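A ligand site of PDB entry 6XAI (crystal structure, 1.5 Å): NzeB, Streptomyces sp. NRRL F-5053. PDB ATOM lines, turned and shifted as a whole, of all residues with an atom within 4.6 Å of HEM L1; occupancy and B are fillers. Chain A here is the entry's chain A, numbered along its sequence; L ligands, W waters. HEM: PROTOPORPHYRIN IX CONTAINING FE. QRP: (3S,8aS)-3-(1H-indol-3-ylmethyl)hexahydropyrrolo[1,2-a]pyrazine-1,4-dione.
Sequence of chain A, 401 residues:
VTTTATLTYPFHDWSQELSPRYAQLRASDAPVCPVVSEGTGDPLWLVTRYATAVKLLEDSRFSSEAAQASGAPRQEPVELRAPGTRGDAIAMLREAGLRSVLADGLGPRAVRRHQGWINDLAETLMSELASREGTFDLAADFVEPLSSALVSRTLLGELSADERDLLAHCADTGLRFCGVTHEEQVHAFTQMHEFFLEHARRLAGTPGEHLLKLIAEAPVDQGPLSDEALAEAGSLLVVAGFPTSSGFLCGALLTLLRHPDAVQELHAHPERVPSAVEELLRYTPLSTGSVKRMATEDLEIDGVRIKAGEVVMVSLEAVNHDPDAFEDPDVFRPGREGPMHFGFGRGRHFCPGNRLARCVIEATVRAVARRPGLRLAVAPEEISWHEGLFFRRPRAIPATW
The backbone NH of Cys 351 is in hydrogen-bond range of the backbone carbonyl oxygen of Phe 344 (3.0 Å).
The backbone NH (N) of Gly 353 sits close to the side-chain sulfur (SG) of Cys 351, 3.2 Å away.
The backbone carbonyl oxygen (O) of Ala 240 sits at hydrogen-bond distance from the side-chain hydroxyl (OG1) of Thr 244 (2.7 Å).
The backbone carbonyl oxygen (O) of Gly 241 is in hydrogen-bond range of the side-chain hydroxyl (OG) of Ser 245 (2.9 Å).
The backbone carbonyl oxygen (O) of Gly 241 sits close to the side-chain hydroxyl (OG1) of Thr 244.
The backbone carbonyl oxygen (O) of Ala 240 lies close to a nitrogen (NC) of HEM L1 (3.3 Å).
Residues that only touch HEM L1: Phe 344 (3.3 Å), Gly 345 (3.4 Å), Leu 316 (3.4 Å), Ser 245 (3.4 Å), Leu 286 (3.5 Å), Gly 343 (3.5 Å), Pro 352 (3.5 Å), Phe 248 (3.5 Å), Val 291 (3.6 Å), Ile 90 (3.6 Å), Leu 106 (3.7 Å), Thr 244 (3.7 Å), Ala 357 (3.7 Å), Gly 241 (3.7 Å), Leu 237 (3.9 Å) and Ile 361 (3.9 Å).
Within 4 Å of HEM L1: Ile 90, Leu 106, Leu 237, Ala 240, Gly 241, Thr 244, Ser 245, Phe 248, Leu 286, Val 291, Arg 293, Leu 316, Gly 343, Phe 344, Gly 345, His 349, Cys 351, Pro 352, Ala 357 and Ile 361.
Water W4 lies within hydrogen-bond range of O2A of HEM L1, O of QRP L3 and NH1 of Arg 293.
Water W2 bridges the side-chain hydroxyl (OG) of Ser 64 (2.6 Å) and an oxygen (O2A) of HEM L1 (2.7 Å).
Water W1 lies within hydrogen-bond range of O1A of HEM L1 and O of His 349.
Water W3 lies within hydrogen-bond range of the backbone carbonyl oxygen (O) of Ala 240 (2.7 Å) and a nitrogen (NE1) of QRP L2 (3.0 Å).
N of QRP L2 lies within hydrogen-bond range of O1D of HEM L1 (2.9 Å).
FE of HEM L1 is bound by SG of Cys 351 (2.3 Å).
An oxygen (O2D) of HEM L1 sits at hydrogen-bond distance from a ring nitrogen (ND1) of His 349, 2.7 Å away.
O1A of HEM L1 is in salt-bridge range of NH2 of Arg 293, 2.8 Å away.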
ATOM      1  N   SER A  64      -2.643   3.094  31.274  1.00  0.00           N
ATOM      2  CA  SER A  64      -1.695   2.040  30.923  1.00  0.00           C
ATOM      3  C   SER A  64      -1.461   1.104  32.105  1.00  0.00           C
ATOM      4  O   SER A  64      -1.459  -0.128  31.937  1.00  0.00           O
ATOM      5  CB  SER A  64      -0.377   2.642  30.450  1.00  0.00           C
ATOM      6  OG  SER A  64       0.555   1.599  30.234  1.00  0.00           O
ATOM      7  N   ILE A  90       7.903   1.452  37.520  1.00  0.00           N
ATOM      8  CA  ILE A  90       7.848   2.913  37.451  1.00  0.00           C
ATOM      9  C   ILE A  90       7.190   3.486  38.713  1.00  0.00           C
ATOM     10  O   ILE A  90       7.651   4.482  39.273  1.00  0.00           O
ATOM     11  CB  ILE A  90       7.150   3.373  36.162  1.00  0.00           C
ATOM     12  CG1 ILE A  90       8.076   3.140  34.968  1.00  0.00           C
ATOM     13  CG2 ILE A  90       6.784   4.849  36.259  1.00  0.00           C
ATOM     14  CD1 ILE A  90       7.378   3.230  33.611  1.00  0.00           C
ATOM     15  N   LEU A 102      14.537   8.042  35.939  1.00  0.00           N
ATOM     16  CA  LEU A 102      14.478   7.438  34.615  1.00  0.00           C
ATOM     17  C   LEU A 102      14.715   8.484  33.534  1.00  0.00           C
ATOM     18  O   LEU A 102      15.601   8.314  32.677  1.00  0.00           O
ATOM     19  CB  LEU A 102      13.119   6.763  34.405  1.00  0.00           C
ATOM     20  CG  LEU A 102      12.940   5.341  34.912  1.00  0.00           C
ATOM     21  CD1 LEU A 102      11.700   4.715  34.277  1.00  0.00           C
ATOM     22  CD2 LEU A 102      14.183   4.512  34.606  1.00  0.00           C
ATOM     23  N   LEU A 106      18.148   9.017  30.907  1.00  0.00           N
ATOM     24  CA  LEU A 106      17.910   8.689  29.515  1.00  0.00           C
ATOM     25  C   LEU A 106      17.705   9.931  28.648  1.00  0.00           C
ATOM     26  O   LEU A 106      17.551   9.806  27.426  1.00  0.00           O
ATOM     27  CB  LEU A 106      16.681   7.772  29.395  1.00  0.00           C
ATOM     28  CG  LEU A 106      16.786   6.398  30.090  1.00  0.00           C
ATOM     29  CD1 LEU A 106      15.436   5.706  30.152  1.00  0.00           C
ATOM     30  CD2 LEU A 106      17.813   5.491  29.414  1.00  0.00           C
ATOM     31  N   LEU A 155      22.684   1.098  31.392  1.00  0.00           N
ATOM     32  CA  LEU A 155      21.550   0.570  32.139  1.00  0.00           C
ATOM     33  C   LEU A 155      21.937  -0.164  33.417  1.00  0.00           C
ATOM     34  O   LEU A 155      21.556   0.281  34.501  1.00  0.00           O
ATOM     35  CB  LEU A 155      20.675  -0.326  31.237  1.00  0.00           C
ATOM     36  CG  LEU A 155      20.124   0.316  29.966  1.00  0.00           C
ATOM     37  CD1 LEU A 155      19.153  -0.630  29.279  1.00  0.00           C
ATOM     38  CD2 LEU A 155      19.468   1.659  30.278  1.00  0.00           C
ATOM     39  N   LEU A 236      12.811  -4.091  34.859  1.00  0.00           N
ATOM     40  CA  LEU A 236      12.280  -3.090  33.924  1.00  0.00           C
ATOM     41  C   LEU A 236      13.314  -2.719  32.875  1.00  0.00           C
ATOM     42  O   LEU A 236      13.010  -2.653  31.671  1.00  0.00           O
ATOM     43  CB  LEU A 236      11.835  -1.843  34.685  1.00  0.00           C
ATOM     44  CG  LEU A 236      11.453  -0.683  33.762  1.00  0.00           C
ATOM     45  CD1 LEU A 236      10.244  -1.094  32.911  1.00  0.00           C
ATOM     46  CD2 LEU A 236      11.187   0.568  34.574  1.00  0.00           C
ATOM     47  N   LEU A 237      14.555  -2.456  33.306  1.00  0.00           N
ATOM     48  CA  LEU A 237      15.570  -2.020  32.350  1.00  0.00           C
ATOM     49  C   LEU A 237      15.868  -3.116  31.345  1.00  0.00           C
ATOM     50  O   LEU A 237      16.091  -2.830  30.157  1.00  0.00           O
ATOM     51  CB  LEU A 237      16.837  -1.572  33.090  1.00  0.00           C
ATOM     52  CG  LEU A 237      16.569  -0.384  34.029  1.00  0.00           C
ATOM     53  CD1 LEU A 237      17.735  -0.114  34.990  1.00  0.00           C
ATOM     54  CD2 LEU A 237      16.233   0.860  33.236  1.00  0.00           C
ATOM     55  N   ALA A 240      12.573  -3.455  29.002  1.00  0.00           N
ATOM     56  CA  ALA A 240      12.306  -2.256  28.217  1.00  0.00           C
ATOM     57  C   ALA A 240      13.451  -1.854  27.308  1.00  0.00           C
ATOM     58  O   ALA A 240      13.223  -1.168  26.303  1.00  0.00           O
ATOM     59  CB  ALA A 240      11.923  -1.078  29.127  1.00  0.00           C
ATOM     60  N   GLY A 241      14.678  -2.247  27.651  1.00  0.00           N
ATOM     61  CA  GLY A 241      15.836  -1.726  26.953  1.00  0.00           C
ATOM     62  C   GLY A 241      16.577  -2.748  26.124  1.00  0.00           C
ATOM     63  O   GLY A 241      17.237  -2.387  25.143  1.00  0.00           O
ATOM     64  N   THR A 244      14.107  -4.633  22.912  1.00  0.00           N
ATOM     65  CA  THR A 244      13.703  -3.522  22.066  1.00  0.00           C
ATOM     66  C   THR A 244      14.881  -3.006  21.252  1.00  0.00           C
ATOM     67  O   THR A 244      14.808  -2.890  20.017  1.00  0.00           O
ATOM     68  CB  THR A 244      13.149  -2.390  22.943  1.00  0.00           C
ATOM     69  OG1 THR A 244      14.103  -2.100  23.978  1.00  0.00           O
ATOM     70  CG2 THR A 244      11.822  -2.802  23.575  1.00  0.00           C
ATOM     71  N   SER A 245      15.991  -2.697  21.924  1.00  0.00           N
ATOM     72  CA  SER A 245      17.148  -2.146  21.210  1.00  0.00           C
ATOM     73  C   SER A 245      17.760  -3.166  20.258  1.00  0.00           C
ATOM     74  O   SER A 245      18.055  -2.843  19.101  1.00  0.00           O
ATOM     75  CB  SER A 245      18.174  -1.632  22.196  1.00  0.00           C
ATOM     76  OG  SER A 245      17.631  -0.545  22.925  1.00  0.00           O
ATOM     77  N   PHE A 248      15.267  -3.711  17.339  1.00  0.00           N
ATOM     78  CA  PHE A 248      15.126  -2.596  16.415  1.00  0.00           C
ATOM     79  C   PHE A 248      16.383  -2.400  15.581  1.00  0.00           C
ATOM     80  O   PHE A 248      16.304  -2.140  14.379  1.00  0.00           O
ATOM     81  CB  PHE A 248      14.721  -1.279  17.081  1.00  0.00           C
ATOM     82  CG  PHE A 248      14.397  -0.228  16.078  1.00  0.00           C
ATOM     83  CD1 PHE A 248      13.138  -0.170  15.511  1.00  0.00           C
ATOM     84  CD2 PHE A 248      15.380   0.617  15.613  1.00  0.00           C
ATOM     85  CE1 PHE A 248      12.867   0.735  14.529  1.00  0.00           C
ATOM     86  CE2 PHE A 248      15.105   1.537  14.639  1.00  0.00           C
ATOM     87  CZ  PHE A 248      13.838   1.596  14.104  1.00  0.00           C
ATOM     88  N   LEU A 281      12.141   4.550  12.303  1.00  0.00           N
ATOM     89  CA  LEU A 281      11.224   4.328  13.413  1.00  0.00           C
ATOM     90  C   LEU A 281       9.770   4.190  12.953  1.00  0.00           C
ATOM     91  O   LEU A 281       8.968   3.536  13.636  1.00  0.00           O
ATOM     92  CB  LEU A 281      11.370   5.448  14.449  1.00  0.00           C
ATOM     93  CG  LEU A 281      12.661   5.382  15.271  1.00  0.00           C
ATOM     94  CD1 LEU A 281      13.019   6.759  15.800  1.00  0.00           C
ATOM     95  CD2 LEU A 281      12.484   4.371  16.396  1.00  0.00           C
ATOM     96  N   LEU A 286       8.564  -3.363  14.853  1.00  0.00           N
ATOM     97  CA  LEU A 286       9.251  -3.882  16.033  1.00  0.00           C
ATOM     98  C   LEU A 286       8.361  -4.842  16.807  1.00  0.00           C
ATOM     99  O   LEU A 286       8.496  -6.070  16.667  1.00  0.00           O
ATOM    100  CB  LEU A 286       9.773  -2.753  16.917  1.00  0.00           C
ATOM    101  CG  LEU A 286      10.570  -3.222  18.140  1.00  0.00           C
ATOM    102  CD1 LEU A 286      11.720  -4.200  17.810  1.00  0.00           C
ATOM    103  CD2 LEU A 286      11.082  -2.014  18.937  1.00  0.00           C
ATOM    104  N   VAL A 291       0.576  -1.680  22.011  1.00  0.00           N
ATOM    105  CA  VAL A 291       0.419  -0.915  23.236  1.00  0.00           C
ATOM    106  C   VAL A 291      -1.028  -1.062  23.678  1.00  0.00           C
ATOM    107  O   VAL A 291      -1.923  -1.281  22.856  1.00  0.00           O
ATOM    108  CB  VAL A 291       0.791   0.560  23.058  1.00  0.00           C
ATOM    109  CG1 VAL A 291       2.231   0.725  22.593  1.00  0.00           C
ATOM    110  CG2 VAL A 291      -0.167   1.240  22.110  1.00  0.00           C
ATOM    111  N   ARG A 293      -4.266  -0.027  26.834  1.00  0.00           N
ATOM    112  CA  ARG A 293      -4.755   0.873  27.872  1.00  0.00           C
ATOM    113  C   ARG A 293      -6.109   0.347  28.336  1.00  0.00           C
ATOM    114  O   ARG A 293      -6.886  -0.152  27.531  1.00  0.00           O
ATOM    115  CB  ARG A 293      -4.958   2.289  27.321  1.00  0.00           C
ATOM    116  CG  ARG A 293      -3.739   2.925  26.682  1.00  0.00           C
ATOM    117  CD  ARG A 293      -2.667   3.270  27.716  1.00  0.00           C
ATOM    118  NE  ARG A 293      -1.563   4.040  27.131  1.00  0.00           N
ATOM    119  CZ  ARG A 293      -0.407   3.517  26.704  1.00  0.00           C
ATOM    120  NH1 ARG A 293      -0.159   2.194  26.772  1.00  0.00           N
ATOM    121  NH2 ARG A 293       0.502   4.321  26.189  1.00  0.00           N
ATOM    122  N   LEU A 316       1.229  -0.252  16.857  1.00  0.00           N
ATOM    123  CA  LEU A 316       2.032   0.858  16.358  1.00  0.00           C
ATOM    124  C   LEU A 316       2.397   0.634  14.898  1.00  0.00           C
ATOM    125  O   LEU A 316       2.477   1.588  14.114  1.00  0.00           O
ATOM    126  CB  LEU A 316       3.284   1.021  17.201  1.00  0.00           C
ATOM    127  CG  LEU A 316       3.009   1.220  18.691  1.00  0.00           C
ATOM    128  CD1 LEU A 316       4.323   1.460  19.414  1.00  0.00           C
ATOM    129  CD2 LEU A 316       2.059   2.383  18.916  1.00  0.00           C
ATOM    130  N   GLY A 343       6.515   5.161  16.415  1.00  0.00           N
ATOM    131  CA  GLY A 343       7.519   4.157  16.800  1.00  0.00           C
ATOM    132  C   GLY A 343       7.882   4.174  18.267  1.00  0.00           C
ATOM    133  O   GLY A 343       8.320   3.143  18.810  1.00  0.00           O
ATOM    134  N   PHE A 344       7.732   5.320  18.925  1.00  0.00           N
ATOM    135  CA  PHE A 344       7.959   5.468  20.367  1.00  0.00           C
ATOM    136  C   PHE A 344       6.654   5.633  21.134  1.00  0.00           C
ATOM    137  O   PHE A 344       6.678   5.954  22.338  1.00  0.00           O
ATOM    138  CB  PHE A 344       8.881   6.668  20.637  1.00  0.00           C
ATOM    139  CG  PHE A 344      10.333   6.455  20.249  1.00  0.00           C
ATOM    140  CD1 PHE A 344      11.049   5.355  20.705  1.00  0.00           C
ATOM    141  CD2 PHE A 344      10.990   7.398  19.468  1.00  0.00           C
ATOM    142  CE1 PHE A 344      12.391   5.181  20.359  1.00  0.00           C
ATOM    143  CE2 PHE A 344      12.330   7.246  19.118  1.00  0.00           C
ATOM    144  CZ  PHE A 344      13.035   6.124  19.560  1.00  0.00           C
ATOM    145  N   GLY A 345       5.508   5.390  20.496  1.00  0.00           N
ATOM    146  CA  GLY A 345       4.219   5.607  21.114  1.00  0.00           C
ATOM    147  C   GLY A 345       3.740   7.042  20.991  1.00  0.00           C
ATOM    148  O   GLY A 345       4.146   7.762  20.063  1.00  0.00           O
ATOM    149  N   HIS A 349       2.975   8.102  27.945  1.00  0.00           N
ATOM    150  CA  HIS A 349       3.922   6.990  28.062  1.00  0.00           C
ATOM    151  C   HIS A 349       4.920   6.930  26.913  1.00  0.00           C
ATOM    152  O   HIS A 349       5.582   5.905  26.731  1.00  0.00           O
ATOM    153  CB  HIS A 349       3.187   5.658  28.243  1.00  0.00           C
ATOM    154  CG  HIS A 349       2.292   5.663  29.448  1.00  0.00           C
ATOM    155  ND1 HIS A 349       2.767   5.490  30.727  1.00  0.00           N
ATOM    156  CD2 HIS A 349       0.951   5.897  29.574  1.00  0.00           C
ATOM    157  CE1 HIS A 349       1.770   5.569  31.582  1.00  0.00           C
ATOM    158  NE2 HIS A 349       0.656   5.832  30.915  1.00  0.00           N
ATOM    159  N   CYS A 351       8.047   6.759  24.841  1.00  0.00           N
ATOM    160  CA  CYS A 351       9.248   6.077  25.300  1.00  0.00           C
ATOM    161  C   CYS A 351      10.197   7.011  26.035  1.00  0.00           C
ATOM    162  O   CYS A 351      10.737   7.944  25.423  1.00  0.00           O
ATOM    163  CB  CYS A 351       9.972   5.464  24.098  1.00  0.00           C
ATOM    164  SG  CYS A 351      11.570   4.739  24.600  1.00  0.00           S
ATOM    165  N   PRO A 352      10.430   6.820  27.330  1.00  0.00           N
ATOM    166  CA  PRO A 352      11.387   7.699  28.035  1.00  0.00           C
ATOM    167  C   PRO A 352      12.818   7.469  27.602  1.00  0.00           C
ATOM    168  O   PRO A 352      13.672   8.330  27.861  1.00  0.00           O
ATOM    169  CB  PRO A 352      11.170   7.358  29.513  1.00  0.00           C
ATOM    170  CG  PRO A 352      10.507   6.031  29.525  1.00  0.00           C
ATOM    171  CD  PRO A 352       9.691   5.935  28.258  1.00  0.00           C
ATOM    172  N   GLY A 353      13.109   6.358  26.933  1.00  0.00           N
ATOM    173  CA  GLY A 353      14.444   6.126  26.403  1.00  0.00           C
ATOM    174  C   GLY A 353      14.628   6.591  24.977  1.00  0.00           C
ATOM    175  O   GLY A 353      15.614   6.236  24.338  1.00  0.00           O
ATOM    176  N   LEU A 356      18.022   8.138  23.917  1.00  0.00           N
ATOM    177  CA  LEU A 356      19.106   7.165  23.878  1.00  0.00           C
ATOM    178  C   LEU A 356      18.945   6.208  22.697  1.00  0.00           C
ATOM    179  O   LEU A 356      19.928   5.915  22.004  1.00  0.00           O
ATOM    180  CB  LEU A 356      19.180   6.390  25.199  1.00  0.00           C
ATOM    181  CG  LEU A 356      20.266   5.324  25.345  1.00  0.00           C
ATOM    182  CD1 LEU A 356      21.651   5.974  25.254  1.00  0.00           C
ATOM    183  CD2 LEU A 356      20.134   4.497  26.641  1.00  0.00           C
ATOM    184  N   ALA A 357      17.731   5.716  22.465  1.00  0.00           N
ATOM    185  CA  ALA A 357      17.484   4.899  21.280  1.00  0.00           C
ATOM    186  C   ALA A 357      17.854   5.642  19.991  1.00  0.00           C
ATOM    187  O   ALA A 357      18.555   5.109  19.129  1.00  0.00           O
ATOM    188  CB  ALA A 357      16.014   4.476  21.245  1.00  0.00           C
ATOM    189  N   ILE A 361      20.576   4.400  17.240  1.00  0.00           N
ATOM    190  CA  ILE A 361      20.115   4.189  15.862  1.00  0.00           C
ATOM    191  C   ILE A 361      20.914   5.069  14.914  1.00  0.00           C
ATOM    192  O   ILE A 361      21.356   4.608  13.854  1.00  0.00           O
ATOM    193  CB  ILE A 361      18.604   4.440  15.704  1.00  0.00           C
ATOM    194  CG1 ILE A 361      17.777   3.482  16.569  1.00  0.00           C
ATOM    195  CG2 ILE A 361      18.220   4.316  14.221  1.00  0.00           C
ATOM    196  CD1 ILE A 361      16.316   3.958  16.821  1.00  0.00           C
HETATM  197  CHA HEM L   1       8.127   2.714  26.535  1.00  0.00           C
HETATM  198  CHB HEM L   1       9.683   1.985  21.996  1.00  0.00           C
HETATM  199  CHC HEM L   1      14.206   1.626  23.687  1.00  0.00           C
HETATM  200  CHD HEM L   1      12.664   2.391  28.217  1.00  0.00           C
HETATM  201  C1A HEM L   1       8.126   2.573  25.176  1.00  0.00           C
HETATM  202  C2A HEM L   1       6.983   2.677  24.288  1.00  0.00           C
HETATM  203  C3A HEM L   1       7.441   2.469  23.048  1.00  0.00           C
HETATM  204  C4A HEM L   1       8.872   2.235  23.082  1.00  0.00           C
HETATM  205  CMA HEM L   1       6.600   2.422  21.765  1.00  0.00           C
HETATM  206  CAA HEM L   1       5.527   2.991  24.676  1.00  0.00           C
HETATM  207  CBA HEM L   1       4.744   1.843  25.305  1.00  0.00           C
HETATM  208  CGA HEM L   1       3.321   2.230  25.641  1.00  0.00           C
HETATM  209  O1A HEM L   1       2.852   3.262  25.103  1.00  0.00           O
HETATM  210  O2A HEM L   1       2.663   1.500  26.439  1.00  0.00           O
HETATM  211  C1B HEM L   1      11.048   1.801  22.042  1.00  0.00           C
HETATM  212  C2B HEM L   1      11.928   1.516  20.919  1.00  0.00           C
HETATM  213  C3B HEM L   1      13.187   1.392  21.407  1.00  0.00           C
HETATM  214  C4B HEM L   1      13.113   1.625  22.843  1.00  0.00           C
HETATM  215  CMB HEM L   1      11.445   1.379  19.457  1.00  0.00           C
HETATM  216  CAB HEM L   1      14.510   1.103  20.653  1.00  0.00           C
HETATM  217  CBB HEM L   1      14.688   1.434  19.370  1.00  0.00           C
HETATM  218  C1C HEM L   1      14.189   1.829  25.047  1.00  0.00           C
HETATM  219  C2C HEM L   1      15.362   1.837  25.906  1.00  0.00           C
HETATM  220  C3C HEM L   1      14.943   2.033  27.152  1.00  0.00           C
HETATM  221  C4C HEM L   1      13.492   2.157  27.134  1.00  0.00           C
HETATM  222  CMC HEM L   1      16.808   1.633  25.424  1.00  0.00           C
HETATM  223  CAC HEM L   1      15.905   2.105  28.367  1.00  0.00           C
HETATM  224  CBC HEM L   1      15.482   2.009  29.623  1.00  0.00           C
HETATM  225  C1D HEM L   1      11.289   2.438  28.180  1.00  0.00           C
HETATM  226  C2D HEM L   1      10.391   2.400  29.301  1.00  0.00           C
HETATM  227  C3D HEM L   1       9.125   2.498  28.831  1.00  0.00           C
HETATM  228  C4D HEM L   1       9.204   2.583  27.399  1.00  0.00           C
HETATM  229  CMD HEM L   1      10.863   2.281  30.777  1.00  0.00           C
HETATM  230  CAD HEM L   1       7.792   2.474  29.631  1.00  0.00           C
HETATM  231  CBD HEM L   1       7.203   3.871  29.743  1.00  0.00           C
HETATM  232  CGD HEM L   1       5.843   3.809  30.411  1.00  0.00           C
HETATM  233  O1D HEM L   1       5.170   2.743  30.401  1.00  0.00           O
HETATM  234  O2D HEM L   1       5.404   4.850  30.945  1.00  0.00           O
HETATM  235  NA  HEM L   1       9.252   2.331  24.415  1.00  0.00           N
HETATM  236  NB  HEM L   1      11.803   1.854  23.193  1.00  0.00           N
HETATM  237  NC  HEM L   1      13.067   2.050  25.821  1.00  0.00           N
HETATM  238  ND  HEM L   1      10.525   2.529  27.021  1.00  0.00           N
HETATM  239 FE   HEM L   1      11.205   2.486  25.074  1.00  0.00          FE
HETATM  240  C   QRP L   2       4.134  -2.353  30.191  1.00  0.00           C
HETATM  241  N   QRP L   2       5.328  -0.183  30.510  1.00  0.00           N
HETATM  242  O   QRP L   2       3.267  -3.046  29.681  1.00  0.00           O
HETATM  243  CA  QRP L   2       4.346  -0.941  29.733  1.00  0.00           C
HETATM  244  CB  QRP L   2       4.690  -1.016  28.226  1.00  0.00           C
HETATM  245  CG  QRP L   2       6.063  -1.594  27.928  1.00  0.00           C
HETATM  246  OAA QRP L   2       6.989  -0.019  32.017  1.00  0.00           O
HETATM  247  CAH QRP L   2       6.522  -4.426  31.707  1.00  0.00           C
HETATM  248  CAI QRP L   2       7.089  -2.999  31.733  1.00  0.00           C
HETATM  249  CAJ QRP L   2       5.030  -4.291  31.434  1.00  0.00           C
HETATM  250  CAN QRP L   2       6.109  -0.685  31.473  1.00  0.00           C
HETATM  251  CAT QRP L   2       5.874  -2.093  31.913  1.00  0.00           C
HETATM  252  NAU QRP L   2       4.920  -2.862  31.134  1.00  0.00           N
HETATM  253  CD1 QRP L   2       7.207  -0.844  27.724  1.00  0.00           C
HETATM  254  CD2 QRP L   2       6.440  -2.917  27.765  1.00  0.00           C
HETATM  255  NE1 QRP L   2       8.237  -1.675  27.457  1.00  0.00           N
HETATM  256  CE2 QRP L   2       7.797  -2.957  27.482  1.00  0.00           C
HETATM  257  CE3 QRP L   2       5.689  -4.095  27.845  1.00  0.00           C
HETATM  258  CH2 QRP L   2       7.705  -5.360  27.370  1.00  0.00           C
HETATM  259  CZ2 QRP L   2       8.434  -4.183  27.295  1.00  0.00           C
HETATM  260  CZ3 QRP L   2       6.337  -5.317  27.644  1.00  0.00           C
HETATM  261  C   QRP L   3       3.246  -4.266  25.399  1.00  0.00           C
HETATM  262  N   QRP L   3       4.322  -4.627  23.252  1.00  0.00           N
HETATM  263  O   QRP L   3       2.595  -3.508  26.102  1.00  0.00           O
HETATM  264  CA  QRP L   3       4.216  -3.708  24.384  1.00  0.00           C
HETATM  265  CB  QRP L   3       3.859  -2.305  23.863  1.00  0.00           C
HETATM  266  CG  QRP L   3       4.830  -1.946  22.766  1.00  0.00           C
HETATM  267  OAA QRP L   3       4.616  -6.724  22.436  1.00  0.00           O
HETATM  268  CAH QRP L   3       2.372  -7.776  25.978  1.00  0.00           C
HETATM  269  CAI QRP L   3       3.002  -7.756  24.598  1.00  0.00           C
HETATM  270  CAJ QRP L   3       2.226  -6.307  26.380  1.00  0.00           C
HETATM  271  CAN QRP L   3       4.300  -5.957  23.337  1.00  0.00           C
HETATM  272  CAT QRP L   3       3.916  -6.528  24.676  1.00  0.00           C
HETATM  273  NAU QRP L   3       3.138  -5.596  25.489  1.00  0.00           N
HETATM  274  CD1 QRP L   3       4.502  -1.877  21.420  1.00  0.00           C
HETATM  275  CD2 QRP L   3       6.196  -1.663  22.838  1.00  0.00           C
HETATM  276  NE1 QRP L   3       5.610  -1.539  20.707  1.00  0.00           N
HETATM  277  CE2 QRP L   3       6.650  -1.423  21.546  1.00  0.00           C
HETATM  278  CE3 QRP L   3       7.050  -1.588  23.916  1.00  0.00           C
HETATM  279  CH2 QRP L   3       8.853  -1.042  22.435  1.00  0.00           C
HETATM  280  CZ2 QRP L   3       7.995  -1.097  21.343  1.00  0.00           C
HETATM  281  CZ3 QRP L   3       8.385  -1.290  23.721  1.00  0.00           C
HETATM  282  O   HOH W   1       3.134   5.848  24.335  1.00  0.00           O
HETATM  283  O   HOH W   2       2.727   2.220  29.035  1.00  0.00           O
HETATM  284  O   HOH W   3      10.617  -0.534  26.102  1.00  0.00           O
HETATM  285  O   HOH W   4       1.450  -0.876  26.426  1.00  0.00           O
HETATM  286  O   HOH W   5       3.601   2.228  32.747  1.00  0.00           O
HETATM  287  O   HOH W   6       7.025   6.979  31.280  1.00  0.00           O
